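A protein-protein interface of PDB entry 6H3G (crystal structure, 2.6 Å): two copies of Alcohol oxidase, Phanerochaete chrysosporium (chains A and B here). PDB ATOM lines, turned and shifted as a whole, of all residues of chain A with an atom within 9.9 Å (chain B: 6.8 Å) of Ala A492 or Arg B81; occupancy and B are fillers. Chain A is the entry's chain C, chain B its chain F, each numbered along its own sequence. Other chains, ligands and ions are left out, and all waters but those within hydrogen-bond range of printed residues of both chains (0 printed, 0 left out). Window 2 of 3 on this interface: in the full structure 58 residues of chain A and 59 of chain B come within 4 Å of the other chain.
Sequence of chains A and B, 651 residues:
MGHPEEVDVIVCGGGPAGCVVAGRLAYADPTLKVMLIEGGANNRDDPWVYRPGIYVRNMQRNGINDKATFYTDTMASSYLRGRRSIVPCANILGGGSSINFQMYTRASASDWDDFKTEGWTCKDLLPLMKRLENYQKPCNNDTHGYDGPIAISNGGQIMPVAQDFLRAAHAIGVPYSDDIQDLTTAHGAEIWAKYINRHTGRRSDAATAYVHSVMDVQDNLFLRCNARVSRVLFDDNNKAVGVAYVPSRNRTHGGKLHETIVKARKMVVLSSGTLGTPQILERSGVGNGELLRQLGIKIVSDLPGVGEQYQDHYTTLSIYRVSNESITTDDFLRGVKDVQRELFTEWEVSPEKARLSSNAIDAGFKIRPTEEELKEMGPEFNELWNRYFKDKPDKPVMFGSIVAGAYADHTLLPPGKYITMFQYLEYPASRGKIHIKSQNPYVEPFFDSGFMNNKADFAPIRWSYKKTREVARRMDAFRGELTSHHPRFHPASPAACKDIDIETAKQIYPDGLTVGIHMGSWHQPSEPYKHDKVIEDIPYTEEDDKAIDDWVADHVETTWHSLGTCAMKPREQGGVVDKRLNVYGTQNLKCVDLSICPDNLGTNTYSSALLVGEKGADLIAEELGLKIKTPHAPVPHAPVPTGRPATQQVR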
ATOM      1  N   ARG A 488     -20.737 -29.578   3.762  1.00  0.00           N
ATOM      2  CA  ARG A 488     -21.270 -29.918   2.444  1.00  0.00           C
ATOM      3  C   ARG A 488     -22.786 -30.160   2.526  1.00  0.00           C
ATOM      4  O   ARG A 488     -23.255 -31.304   2.408  1.00  0.00           O
ATOM      5  CB  ARG A 488     -20.520 -31.131   1.885  1.00  0.00           C
ATOM      6  CG  ARG A 488     -19.060 -30.845   1.562  1.00  0.00           C
ATOM      7  CD  ARG A 488     -18.322 -32.093   1.115  1.00  0.00           C
ATOM      8  NE  ARG A 488     -17.024 -31.806   0.520  1.00  0.00           N
ATOM      9  CZ  ARG A 488     -16.217 -32.726  -0.003  1.00  0.00           C
ATOM     10  NH1 ARG A 488     -16.553 -34.006   0.043  1.00  0.00           N
ATOM     11  NH2 ARG A 488     -15.076 -32.361  -0.567  1.00  0.00           N
ATOM     12  N   PHE A 489     -23.540 -29.066   2.708  1.00  0.00           N
ATOM     13  CA  PHE A 489     -24.985 -29.090   2.670  1.00  0.00           C
ATOM     14  C   PHE A 489     -25.458 -29.330   1.235  1.00  0.00           C
ATOM     15  O   PHE A 489     -24.813 -28.882   0.283  1.00  0.00           O
ATOM     16  CB  PHE A 489     -25.560 -27.761   3.163  1.00  0.00           C
ATOM     17  CG  PHE A 489     -25.179 -27.380   4.571  1.00  0.00           C
ATOM     18  CD1 PHE A 489     -25.521 -28.186   5.642  1.00  0.00           C
ATOM     19  CD2 PHE A 489     -24.493 -26.203   4.829  1.00  0.00           C
ATOM     20  CE1 PHE A 489     -25.170 -27.830   6.935  1.00  0.00           C
ATOM     21  CE2 PHE A 489     -24.150 -25.844   6.125  1.00  0.00           C
ATOM     22  CZ  PHE A 489     -24.485 -26.661   7.174  1.00  0.00           C
ATOM     23  N   HIS A 490     -26.599 -30.017   1.095  1.00  0.00           N
ATOM     24  CA  HIS A 490     -27.352 -30.056  -0.156  1.00  0.00           C
ATOM     25  C   HIS A 490     -27.663 -28.621  -0.578  1.00  0.00           C
ATOM     26  O   HIS A 490     -28.146 -27.826   0.229  1.00  0.00           O
ATOM     27  CB  HIS A 490     -28.636 -30.881  -0.010  1.00  0.00           C
ATOM     28  CG  HIS A 490     -29.275 -31.257  -1.309  1.00  0.00           C
ATOM     29  ND1 HIS A 490     -30.099 -30.395  -2.009  1.00  0.00           N
ATOM     30  CD2 HIS A 490     -29.234 -32.401  -2.027  1.00  0.00           C
ATOM     31  CE1 HIS A 490     -30.533 -30.995  -3.102  1.00  0.00           C
ATOM     32  NE2 HIS A 490     -30.020 -32.228  -3.135  1.00  0.00           N
ATOM     33  N   PRO A 491     -27.384 -28.226  -1.841  1.00  0.00           N
ATOM     34  CA  PRO A 491     -27.537 -26.831  -2.258  1.00  0.00           C
ATOM     35  C   PRO A 491     -28.952 -26.259  -2.107  1.00  0.00           C
ATOM     36  O   PRO A 491     -29.109 -25.045  -2.003  1.00  0.00           O
ATOM     37  CB  PRO A 491     -27.161 -26.863  -3.744  1.00  0.00           C
ATOM     38  CG  PRO A 491     -26.256 -28.071  -3.866  1.00  0.00           C
ATOM     39  CD  PRO A 491     -26.862 -29.081  -2.917  1.00  0.00           C
ATOM     40  N   ALA A 492     -29.952 -27.144  -2.115  1.00  0.00           N
ATOM     41  CA  ALA A 492     -31.359 -26.776  -2.036  1.00  0.00           C
ATOM     42  C   ALA A 492     -31.841 -26.682  -0.578  1.00  0.00           C
ATOM     43  O   ALA A 492     -32.930 -26.154  -0.335  1.00  0.00           O
ATOM     44  CB  ALA A 492     -32.179 -27.778  -2.812  1.00  0.00           C
ATOM     45  N   SER A 493     -31.047 -27.201   0.373  1.00  0.00           N
ATOM     46  CA  SER A 493     -31.388 -27.209   1.813  1.00  0.00           C
ATOM     47  C   SER A 493     -31.576 -25.788   2.337  1.00  0.00           C
ATOM     48  O   SER A 493     -30.759 -24.911   2.058  1.00  0.00           O
ATOM     49  CB  SER A 493     -30.329 -27.912   2.622  1.00  0.00           C
ATOM     50  OG  SER A 493     -30.589 -27.784   4.013  1.00  0.00           O
ATOM     51  N   PRO A 494     -32.624 -25.518   3.149  1.00  0.00           N
ATOM     52  CA  PRO A 494     -32.746 -24.225   3.827  1.00  0.00           C
ATOM     53  C   PRO A 494     -31.537 -23.869   4.716  1.00  0.00           C
ATOM     54  O   PRO A 494     -31.387 -22.702   5.100  1.00  0.00           O
ATOM     55  CB  PRO A 494     -34.025 -24.378   4.666  1.00  0.00           C
ATOM     56  CG  PRO A 494     -34.816 -25.441   3.935  1.00  0.00           C
ATOM     57  CD  PRO A 494     -33.767 -26.403   3.419  1.00  0.00           C
ATOM     58  N   ALA A 495     -30.683 -24.865   4.999  1.00  0.00           N
ATOM     59  CA  ALA A 495     -29.479 -24.716   5.832  1.00  0.00           C
ATOM     60  C   ALA A 495     -28.196 -24.534   4.994  1.00  0.00           C
ATOM     61  O   ALA A 495     -27.083 -24.564   5.551  1.00  0.00           O
ATOM     62  CB  ALA A 495     -29.365 -25.924   6.737  1.00  0.00           C
ATOM     63  N   ALA A 496     -28.337 -24.345   3.674  1.00  0.00           N
ATOM     64  CA  ALA A 496     -27.187 -24.194   2.767  1.00  0.00           C
ATOM     65  C   ALA A 496     -26.542 -22.825   2.996  1.00  0.00           C
ATOM     66  O   ALA A 496     -27.224 -21.866   3.376  1.00  0.00           O
ATOM     67  CB  ALA A 496     -27.609 -24.366   1.327  1.00  0.00           C
ATOM     68  N   CYS A 497     -25.232 -22.757   2.745  1.00  0.00           N
ATOM     69  CA  CYS A 497     -24.443 -21.566   2.963  1.00  0.00           C
ATOM     70  C   CYS A 497     -24.811 -20.473   1.955  1.00  0.00           C
ATOM     71  O   CYS A 497     -25.315 -20.755   0.884  1.00  0.00           O
ATOM     72  CB  CYS A 497     -22.962 -21.891   2.849  1.00  0.00           C
ATOM     73  SG  CYS A 497     -22.386 -22.953   4.197  1.00  0.00           S
ATOM     74  N   LYS A 498     -24.543 -19.223   2.328  1.00  0.00           N
ATOM     75  CA  LYS A 498     -24.616 -18.094   1.424  1.00  0.00           C
ATOM     76  C   LYS A 498     -23.324 -17.285   1.546  1.00  0.00           C
ATOM     77  O   LYS A 498     -23.027 -16.753   2.622  1.00  0.00           O
ATOM     78  CB  LYS A 498     -25.828 -17.220   1.749  1.00  0.00           C
ATOM     79  CG  LYS A 498     -27.159 -17.954   1.730  1.00  0.00           C
ATOM     80  CD  LYS A 498     -28.297 -17.122   1.200  1.00  0.00           C
ATOM     81  CE  LYS A 498     -29.607 -17.874   1.219  1.00  0.00           C
ATOM     82  NZ  LYS A 498     -29.691 -18.836   0.094  1.00  0.00           N
ATOM     83  N   SER A 521     -21.832 -21.252 -10.852  1.00  0.00           N
ATOM     84  CA  SER A 521     -22.740 -21.354  -9.706  1.00  0.00           C
ATOM     85  C   SER A 521     -21.994 -21.958  -8.509  1.00  0.00           C
ATOM     86  O   SER A 521     -22.441 -22.935  -7.907  1.00  0.00           O
ATOM     87  CB  SER A 521     -23.958 -22.158 -10.065  1.00  0.00           C
ATOM     88  OG  SER A 521     -24.610 -21.601 -11.192  1.00  0.00           O
ATOM     89  N   GLN A 524     -23.972 -19.401  -3.685  1.00  0.00           N
ATOM     90  CA  GLN A 524     -25.256 -18.708  -3.661  1.00  0.00           C
ATOM     91  C   GLN A 524     -25.046 -17.372  -2.948  1.00  0.00           C
ATOM     92  O   GLN A 524     -24.793 -17.341  -1.746  1.00  0.00           O
ATOM     93  CB  GLN A 524     -26.323 -19.569  -2.974  1.00  0.00           C
ATOM     94  CG  GLN A 524     -26.496 -20.957  -3.582  1.00  0.00           C
ATOM     95  CD  GLN A 524     -27.441 -21.819  -2.776  1.00  0.00           C
ATOM     96  OE1 GLN A 524     -28.384 -21.330  -2.156  1.00  0.00           O
ATOM     97  NE2 GLN A 524     -27.193 -23.121  -2.772  1.00  0.00           N
ATOM     98  N   PRO A 539     -33.372 -23.550  10.061  1.00  0.00           N
ATOM     99  CA  PRO A 539     -33.831 -24.919  10.319  1.00  0.00           C
ATOM    100  C   PRO A 539     -32.853 -25.968   9.771  1.00  0.00           C
ATOM    101  O   PRO A 539     -32.305 -25.754   8.698  1.00  0.00           O
ATOM    102  CB  PRO A 539     -35.165 -25.007   9.571  1.00  0.00           C
ATOM    103  CG  PRO A 539     -35.043 -23.993   8.454  1.00  0.00           C
ATOM    104  CD  PRO A 539     -34.117 -22.906   8.967  1.00  0.00           C
ATOM    105  N   THR A 541     -32.116 -30.408   9.224  1.00  0.00           N
ATOM    106  CA  THR A 541     -32.660 -31.768   9.161  1.00  0.00           C
ATOM    107  C   THR A 541     -31.593 -32.775   9.621  1.00  0.00           C
ATOM    108  O   THR A 541     -30.496 -32.385  10.045  1.00  0.00           O
ATOM    109  CB  THR A 541     -33.151 -32.090   7.742  1.00  0.00           C
ATOM    110  OG1 THR A 541     -32.009 -32.268   6.896  1.00  0.00           O
ATOM    111  CG2 THR A 541     -34.090 -31.035   7.190  1.00  0.00           C
ATOM    112  N   GLU A 543     -30.220 -34.907   7.565  1.00  0.00           N
ATOM    113  CA  GLU A 543     -29.243 -34.913   6.452  1.00  0.00           C
ATOM    114  C   GLU A 543     -28.211 -33.803   6.688  1.00  0.00           C
ATOM    115  O   GLU A 543     -26.998 -34.042   6.621  1.00  0.00           O
ATOM    116  CB  GLU A 543     -29.903 -34.706   5.081  1.00  0.00           C
ATOM    117  CG  GLU A 543     -30.978 -35.722   4.714  1.00  0.00           C
ATOM    118  CD  GLU A 543     -30.733 -37.157   5.149  1.00  0.00           C
ATOM    119  OE1 GLU A 543     -31.412 -37.609   6.094  1.00  0.00           O
ATOM    120  OE2 GLU A 543     -29.879 -37.824   4.533  1.00  0.00           O
ATOM    121  N   ASP A 544     -28.712 -32.594   6.966  1.00  0.00           N
ATOM    122  CA  ASP A 544     -27.879 -31.456   7.362  1.00  0.00           C
ATOM    123  C   ASP A 544     -26.936 -31.865   8.505  1.00  0.00           C
ATOM    124  O   ASP A 544     -25.739 -31.637   8.425  1.00  0.00           O
ATOM    125  CB  ASP A 544     -28.729 -30.258   7.788  1.00  0.00           C
ATOM    126  CG  ASP A 544     -29.611 -29.678   6.693  1.00  0.00           C
ATOM    127  OD1 ASP A 544     -29.150 -29.595   5.527  1.00  0.00           O
ATOM    128  OD2 ASP A 544     -30.752 -29.288   7.020  1.00  0.00           O
ATOM    129  N   ALA B  76     -37.469 -23.749 -10.172  1.00  0.00           N
ATOM    130  CA  ALA B  76     -36.273 -24.485  -9.813  1.00  0.00           C
ATOM    131  C   ALA B  76     -36.320 -25.860 -10.477  1.00  0.00           C
ATOM    132  O   ALA B  76     -37.396 -26.409 -10.731  1.00  0.00           O
ATOM    133  CB  ALA B  76     -36.157 -24.604  -8.314  1.00  0.00           C
ATOM    134  N   SER B  77     -35.138 -26.405 -10.758  1.00  0.00           N
ATOM    135  CA  SER B  77     -35.041 -27.624 -11.506  1.00  0.00           C
ATOM    136  C   SER B  77     -34.581 -28.745 -10.581  1.00  0.00           C
ATOM    137  O   SER B  77     -33.465 -28.704 -10.067  1.00  0.00           O
ATOM    138  CB  SER B  77     -34.107 -27.477 -12.664  1.00  0.00           C
ATOM    139  OG  SER B  77     -33.946 -28.722 -13.319  1.00  0.00           O
ATOM    140  N   SER B  78     -35.442 -29.750 -10.413  1.00  0.00           N
ATOM    141  CA  SER B  78     -35.080 -30.984  -9.731  1.00  0.00           C
ATOM    142  C   SER B  78     -33.800 -31.587 -10.344  1.00  0.00           C
ATOM    143  O   SER B  78     -33.050 -32.249  -9.653  1.00  0.00           O
ATOM    144  CB  SER B  78     -36.239 -31.963  -9.737  1.00  0.00           C
ATOM    145  OG  SER B  78     -36.942 -31.959 -10.977  1.00  0.00           O
ATOM    146  N   TYR B  79     -33.536 -31.316 -11.630  1.00  0.00           N
ATOM    147  CA  TYR B  79     -32.399 -31.895 -12.368  1.00  0.00           C
ATOM    148  C   TYR B  79     -31.070 -31.201 -12.030  1.00  0.00           C
ATOM    149  O   TYR B  79     -30.008 -31.823 -12.154  1.00  0.00           O
ATOM    150  CB  TYR B  79     -32.671 -31.854 -13.872  1.00  0.00           C
ATOM    151  CG  TYR B  79     -33.960 -32.534 -14.255  1.00  0.00           C
ATOM    152  CD1 TYR B  79     -34.040 -33.916 -14.360  1.00  0.00           C
ATOM    153  CD2 TYR B  79     -35.113 -31.796 -14.475  1.00  0.00           C
ATOM    154  CE1 TYR B  79     -35.228 -34.543 -14.699  1.00  0.00           C
ATOM    155  CE2 TYR B  79     -36.308 -32.408 -14.812  1.00  0.00           C
ATOM    156  CZ  TYR B  79     -36.365 -33.786 -14.921  1.00  0.00           C
ATOM    157  OH  TYR B  79     -37.547 -34.381 -15.250  1.00  0.00           O
ATOM    158  N   LEU B  80     -31.120 -29.929 -11.610  1.00  0.00           N
ATOM    159  CA  LEU B  80     -29.905 -29.188 -11.233  1.00  0.00           C
ATOM    160  C   LEU B  80     -29.744 -29.113  -9.701  1.00  0.00           C
ATOM    161  O   LEU B  80     -28.822 -28.459  -9.208  1.00  0.00           O
ATOM    162  CB  LEU B  80     -29.969 -27.794 -11.860  1.00  0.00           C
ATOM    163  CG  LEU B  80     -30.216 -27.748 -13.370  1.00  0.00           C
ATOM    164  CD1 LEU B  80     -30.387 -26.309 -13.841  1.00  0.00           C
ATOM    165  CD2 LEU B  80     -29.095 -28.437 -14.143  1.00  0.00           C
ATOM    166  N   ARG B  81     -30.613 -29.823  -8.966  1.00  0.00           N
ATOM    167  CA  ARG B  81     -30.655 -29.874  -7.491  1.00  0.00           C
ATOM    168  C   ARG B  81     -31.184 -28.544  -6.936  1.00  0.00           C
ATOM    169  O   ARG B  81     -30.628 -27.969  -6.000  1.00  0.00           O
ATOM    170  CB  ARG B  81     -29.302 -30.293  -6.902  1.00  0.00           C
ATOM    171  CG  ARG B  81     -28.926 -31.726  -7.255  1.00  0.00           C
ATOM    172  CD  ARG B  81     -27.497 -32.080  -6.912  1.00  0.00           C
ATOM    173  NE  ARG B  81     -27.383 -32.612  -5.566  1.00  0.00           N
ATOM    174  CZ  ARG B  81     -26.373 -32.381  -4.737  1.00  0.00           C
ATOM    175  NH1 ARG B  81     -25.409 -31.538  -5.067  1.00  0.00           N
ATOM    176  NH2 ARG B  81     -26.337 -32.999  -3.571  1.00  0.00           N
ATOM    177  N   GLY B  82     -32.298 -28.094  -7.521  1.00  0.00           N
ATOM    178  CA  GLY B  82     -33.122 -27.022  -6.982  1.00  0.00           C
ATOM    179  C   GLY B  82     -32.667 -25.634  -7.404  1.00  0.00           C
ATOM    180  O   GLY B  82     -33.196 -24.645  -6.885  1.00  0.00           O
ATOM    181  N   ARG B  83     -31.701 -25.543  -8.331  1.00  0.00           N
ATOM    182  CA  ARG B  83     -31.155 -24.237  -8.712  1.00  0.00           C
ATOM    183  C   ARG B  83     -31.870 -23.737  -9.971  1.00  0.00           C
ATOM    184  O   ARG B  83     -32.182 -24.516 -10.867  1.00  0.00           O
ATOM    185  CB  ARG B  83     -29.628 -24.245  -8.878  1.00  0.00           C
ATOM    186  CG  ARG B  83     -29.054 -25.229  -9.887  1.00  0.00           C
ATOM    187  CD  ARG B  83     -27.532 -25.179  -9.917  1.00  0.00           C
ATOM    188  NE  ARG B  83     -27.007 -24.408 -11.038  1.00  0.00           N
ATOM    189  CZ  ARG B  83     -26.551 -24.922 -12.186  1.00  0.00           C
ATOM    190  NH1 ARG B  83     -26.537 -26.231 -12.384  1.00  0.00           N
ATOM    191  NH2 ARG B  83     -26.100 -24.121 -13.135  1.00  0.00           N
ATOM    192  N   ARG B 488     -17.273 -33.014  -4.815  1.00  0.00           N
ATOM    193  CA  ARG B 488     -17.169 -33.357  -3.401  1.00  0.00           C
ATOM    194  C   ARG B 488     -16.835 -34.850  -3.243  1.00  0.00           C
ATOM    195  O   ARG B 488     -17.683 -35.665  -2.891  1.00  0.00           O
ATOM    196  CB  ARG B 488     -18.475 -32.967  -2.703  1.00  0.00           C
ATOM    197  CG  ARG B 488     -18.801 -31.481  -2.783  1.00  0.00           C
ATOM    198  CD  ARG B 488     -20.183 -31.192  -2.221  1.00  0.00           C
ATOM    199  NE  ARG B 488     -20.411 -29.818  -1.782  1.00  0.00           N
ATOM    200  CZ  ARG B 488     -21.574 -29.399  -1.292  1.00  0.00           C
ATOM    201  NH1 ARG B 488     -22.567 -30.265  -1.169  1.00  0.00           N
ATOM    202  NH2 ARG B 488     -21.752 -28.137  -0.932  1.00  0.00           N
ATOM    203  N   LYS B 546     -20.737 -40.629  -8.698  1.00  0.00           N
ATOM    204  CA  LYS B 546     -21.974 -40.025  -8.217  1.00  0.00           C
ATOM    205  C   LYS B 546     -21.674 -38.616  -7.697  1.00  0.00           C
ATOM    206  O   LYS B 546     -22.524 -37.728  -7.787  1.00  0.00           O
ATOM    207  CB  LYS B 546     -22.643 -40.902  -7.155  1.00  0.00           C
ATOM    208  CG  LYS B 546     -24.150 -40.699  -7.017  1.00  0.00           C
ATOM    209  CD  LYS B 546     -24.546 -39.760  -5.897  1.00  0.00           C
ATOM    210  CE  LYS B 546     -26.013 -39.382  -5.920  1.00  0.00           C
ATOM    211  NZ  LYS B 546     -26.407 -38.658  -4.686  1.00  0.00           N
ATOM    212  N   ALA B 547     -20.459 -38.426  -7.168  1.00  0.00           N
ATOM    213  CA  ALA B 547     -20.006 -37.114  -6.742  1.00  0.00           C
ATOM    214  C   ALA B 547     -19.990 -36.176  -7.956  1.00  0.00           C
ATOM    215  O   ALA B 547     -20.503 -35.065  -7.876  1.00  0.00           O
ATOM    216  CB  ALA B 547     -18.655 -37.205  -6.068  1.00  0.00           C
ATOM    217  N   ASP B 549     -21.545 -36.461 -10.897  1.00  0.00           N
ATOM    218  CA  ASP B 549     -22.911 -36.233 -11.397  1.00  0.00           C
ATOM    219  C   ASP B 549     -23.581 -35.107 -10.599  1.00  0.00           C
ATOM    220  O   ASP B 549     -24.351 -34.327 -11.136  1.00  0.00           O
ATOM    221  CB  ASP B 549     -23.758 -37.507 -11.337  1.00  0.00           C
ATOM    222  CG  ASP B 549     -23.295 -38.621 -12.268  1.00  0.00           C
ATOM    223  OD1 ASP B 549     -22.594 -38.318 -13.263  1.00  0.00           O
ATOM    224  OD2 ASP B 549     -23.639 -39.792 -11.990  1.00  0.00           O
ATOM    225  N   ASP B 550     -23.293 -35.049  -9.300  1.00  0.00           N
ATOM    226  CA  ASP B 550     -23.784 -33.981  -8.433  1.00  0.00           C
ATOM    227  C   ASP B 550     -23.156 -32.646  -8.858  1.00  0.00           C
ATOM    228  O   ASP B 550     -23.863 -31.642  -8.998  1.00  0.00           O
ATOM    229  CB  ASP B 550     -23.506 -34.293  -6.958  1.00  0.00           C
ATOM    230  CG  ASP B 550     -24.451 -35.318  -6.355  1.00  0.00           C
ATOM    231  OD1 ASP B 550     -24.934 -36.195  -7.107  1.00  0.00           O
ATOM    232  OD2 ASP B 550     -24.707 -35.222  -5.144  1.00  0.00           O
ATOM    233  N   TRP B 551     -21.830 -32.658  -9.051  1.00  0.00           N
ATOM    234  CA  TRP B 551     -21.031 -31.487  -9.458  1.00  0.00           C
ATOM    235  C   TRP B 551     -21.528 -30.932 -10.803  1.00  0.00           C
ATOM    236  O   TRP B 551     -21.601 -29.721 -11.002  1.00  0.00           O
ATOM    237  CB  TRP B 551     -19.549 -31.877  -9.509  1.00  0.00           C
ATOM    238  CG  TRP B 551     -18.597 -30.795  -9.919  1.00  0.00           C
ATOM    239  CD1 TRP B 551     -17.972 -29.890  -9.111  1.00  0.00           C
ATOM    240  CD2 TRP B 551     -18.102 -30.548 -11.244  1.00  0.00           C
ATOM    241  NE1 TRP B 551     -17.146 -29.081  -9.844  1.00  0.00           N
ATOM    242  CE2 TRP B 551     -17.204 -29.460 -11.154  1.00  0.00           C
ATOM    243  CE3 TRP B 551     -18.349 -31.124 -12.494  1.00  0.00           C
ATOM    244  CZ2 TRP B 551     -16.547 -28.945 -12.267  1.00  0.00           C
ATOM    245  CZ3 TRP B 551     -17.697 -30.616 -13.593  1.00  0.00           C
ATOM    246  CH2 TRP B 551     -16.811 -29.542 -13.478  1.00  0.00           C
ATOM    247  N   ALA B 553     -24.642 -31.362 -11.970  1.00  0.00           N
ATOM    248  CA  ALA B 553     -25.986 -30.808 -11.764  1.00  0.00           C
ATOM    249  C   ALA B 553     -25.890 -29.443 -11.075  1.00  0.00           C
ATOM    250  O   ALA B 553     -26.707 -28.560 -11.315  1.00  0.00           O
ATOM    251  CB  ALA B 553     -26.825 -31.764 -10.957  1.00  0.00           C
ATOM    252  N   ASP B 554     -24.873 -29.294 -10.220  1.00  0.00           N
ATOM    253  CA  ASP B 554     -24.662 -28.093  -9.424  1.00  0.00           C
ATOM    254  C   ASP B 554     -24.092 -26.952 -10.274  1.00  0.00           C
ATOM    255  O   ASP B 554     -24.490 -25.795 -10.073  1.00  0.00           O
ATOM    256  CB  ASP B 554     -23.722 -28.367  -8.246  1.00  0.00           C
ATOM    257  CG  ASP B 554     -24.361 -29.199  -7.153  1.00  0.00           C
ATOM    258  OD1 ASP B 554     -25.599 -29.275  -7.134  1.00  0.00           O
ATOM    259  OD2 ASP B 554     -23.615 -29.762  -6.331  1.00  0.00           O
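Among the printed residues, pairs that only touch across the chains: His A490 with Arg B81, Arg A488 with Arg B488, Ser A521 with Arg B83, Pro A491 with Asp B554, Ala A492 with Arg B81, Pro A491 with Arg B81 and Ser A521 with Asp B554.
The backbone carbonyl oxygen (O) of Phe A489 sits at hydrogen-bond distance from the guanidinium group (NH1) of Arg B488 (3.0 Å).
Arg B488 touches its own counterpart, Arg A488.
Position printed for both chains: 488.
Printed residues of chain B within 4 Å of Phe A489: Arg B488 (3.0 Å).
Ala A492 touches just one residue of chain B: Arg B81 (3.6 Å).
Ser A493 touches none of the printed residues of chain B.
Printed residues of chain B within 4 Å of Ser A521: Arg B83 (3.5 Å) and Asp B554 (3.7 Å).
Tyr B79 touches none of the printed residues of chain A.
Arg B81 touches three residues of chain A.
Printed residues of chain A within 4 Å of Arg B83: Ser A521.
Printed residues of chain A within 4 Å of Arg B488: Arg A488 and Phe A489.
No residue of chain A comes within 4 Å of Asp B550.
Of the printed residues of chain A, Asp B554 touches Pro A491 and Ser A521.
The nearest residue of chain B that does not touch Ala A492 is Gly B82 (4.3 Å).
The nearest printed residue of chain B that does not touch Pro A491 is Arg B488 (4.8 Å).
Of the 16 printed residues of chain B, 4 touch a printed residue of chain A.
Printed residues of chain B that touch a printed residue of chain A: Arg B81, Arg B83, Arg B488 and Asp B554.
Of the 17 printed residues of chain A, 6 touch a printed residue of chain B.
Among the printed residues, no Asp or Glu carboxylate lies within 4 Å of a Lys or Arg side-chain nitrogen of the other chain.
N of Ala A492 lies close to ND1 of His A490 (3.3 Å).
The side-chain amide nitrogen (NE2) of Gln A524 lies within hydrogen-bond range of the backbone carbonyl oxygen (O) of Pro A491 (2.8 Å).
OD2 of Asp B550 lies within salt-bridge range of NH2 of Arg B81, 3.2 Å away.
The guanidinium group of Arg B81 lies within salt-bridge range of the side-chain carboxylate of Asp B554 (2.8 Å).
O of Ala B553 sits at hydrogen-bond distance from NH1 of Arg B83 (2.6 Å).
NE of Arg B83 sits at hydrogen-bond distance from O of Asp B554, 3.0 Å away.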
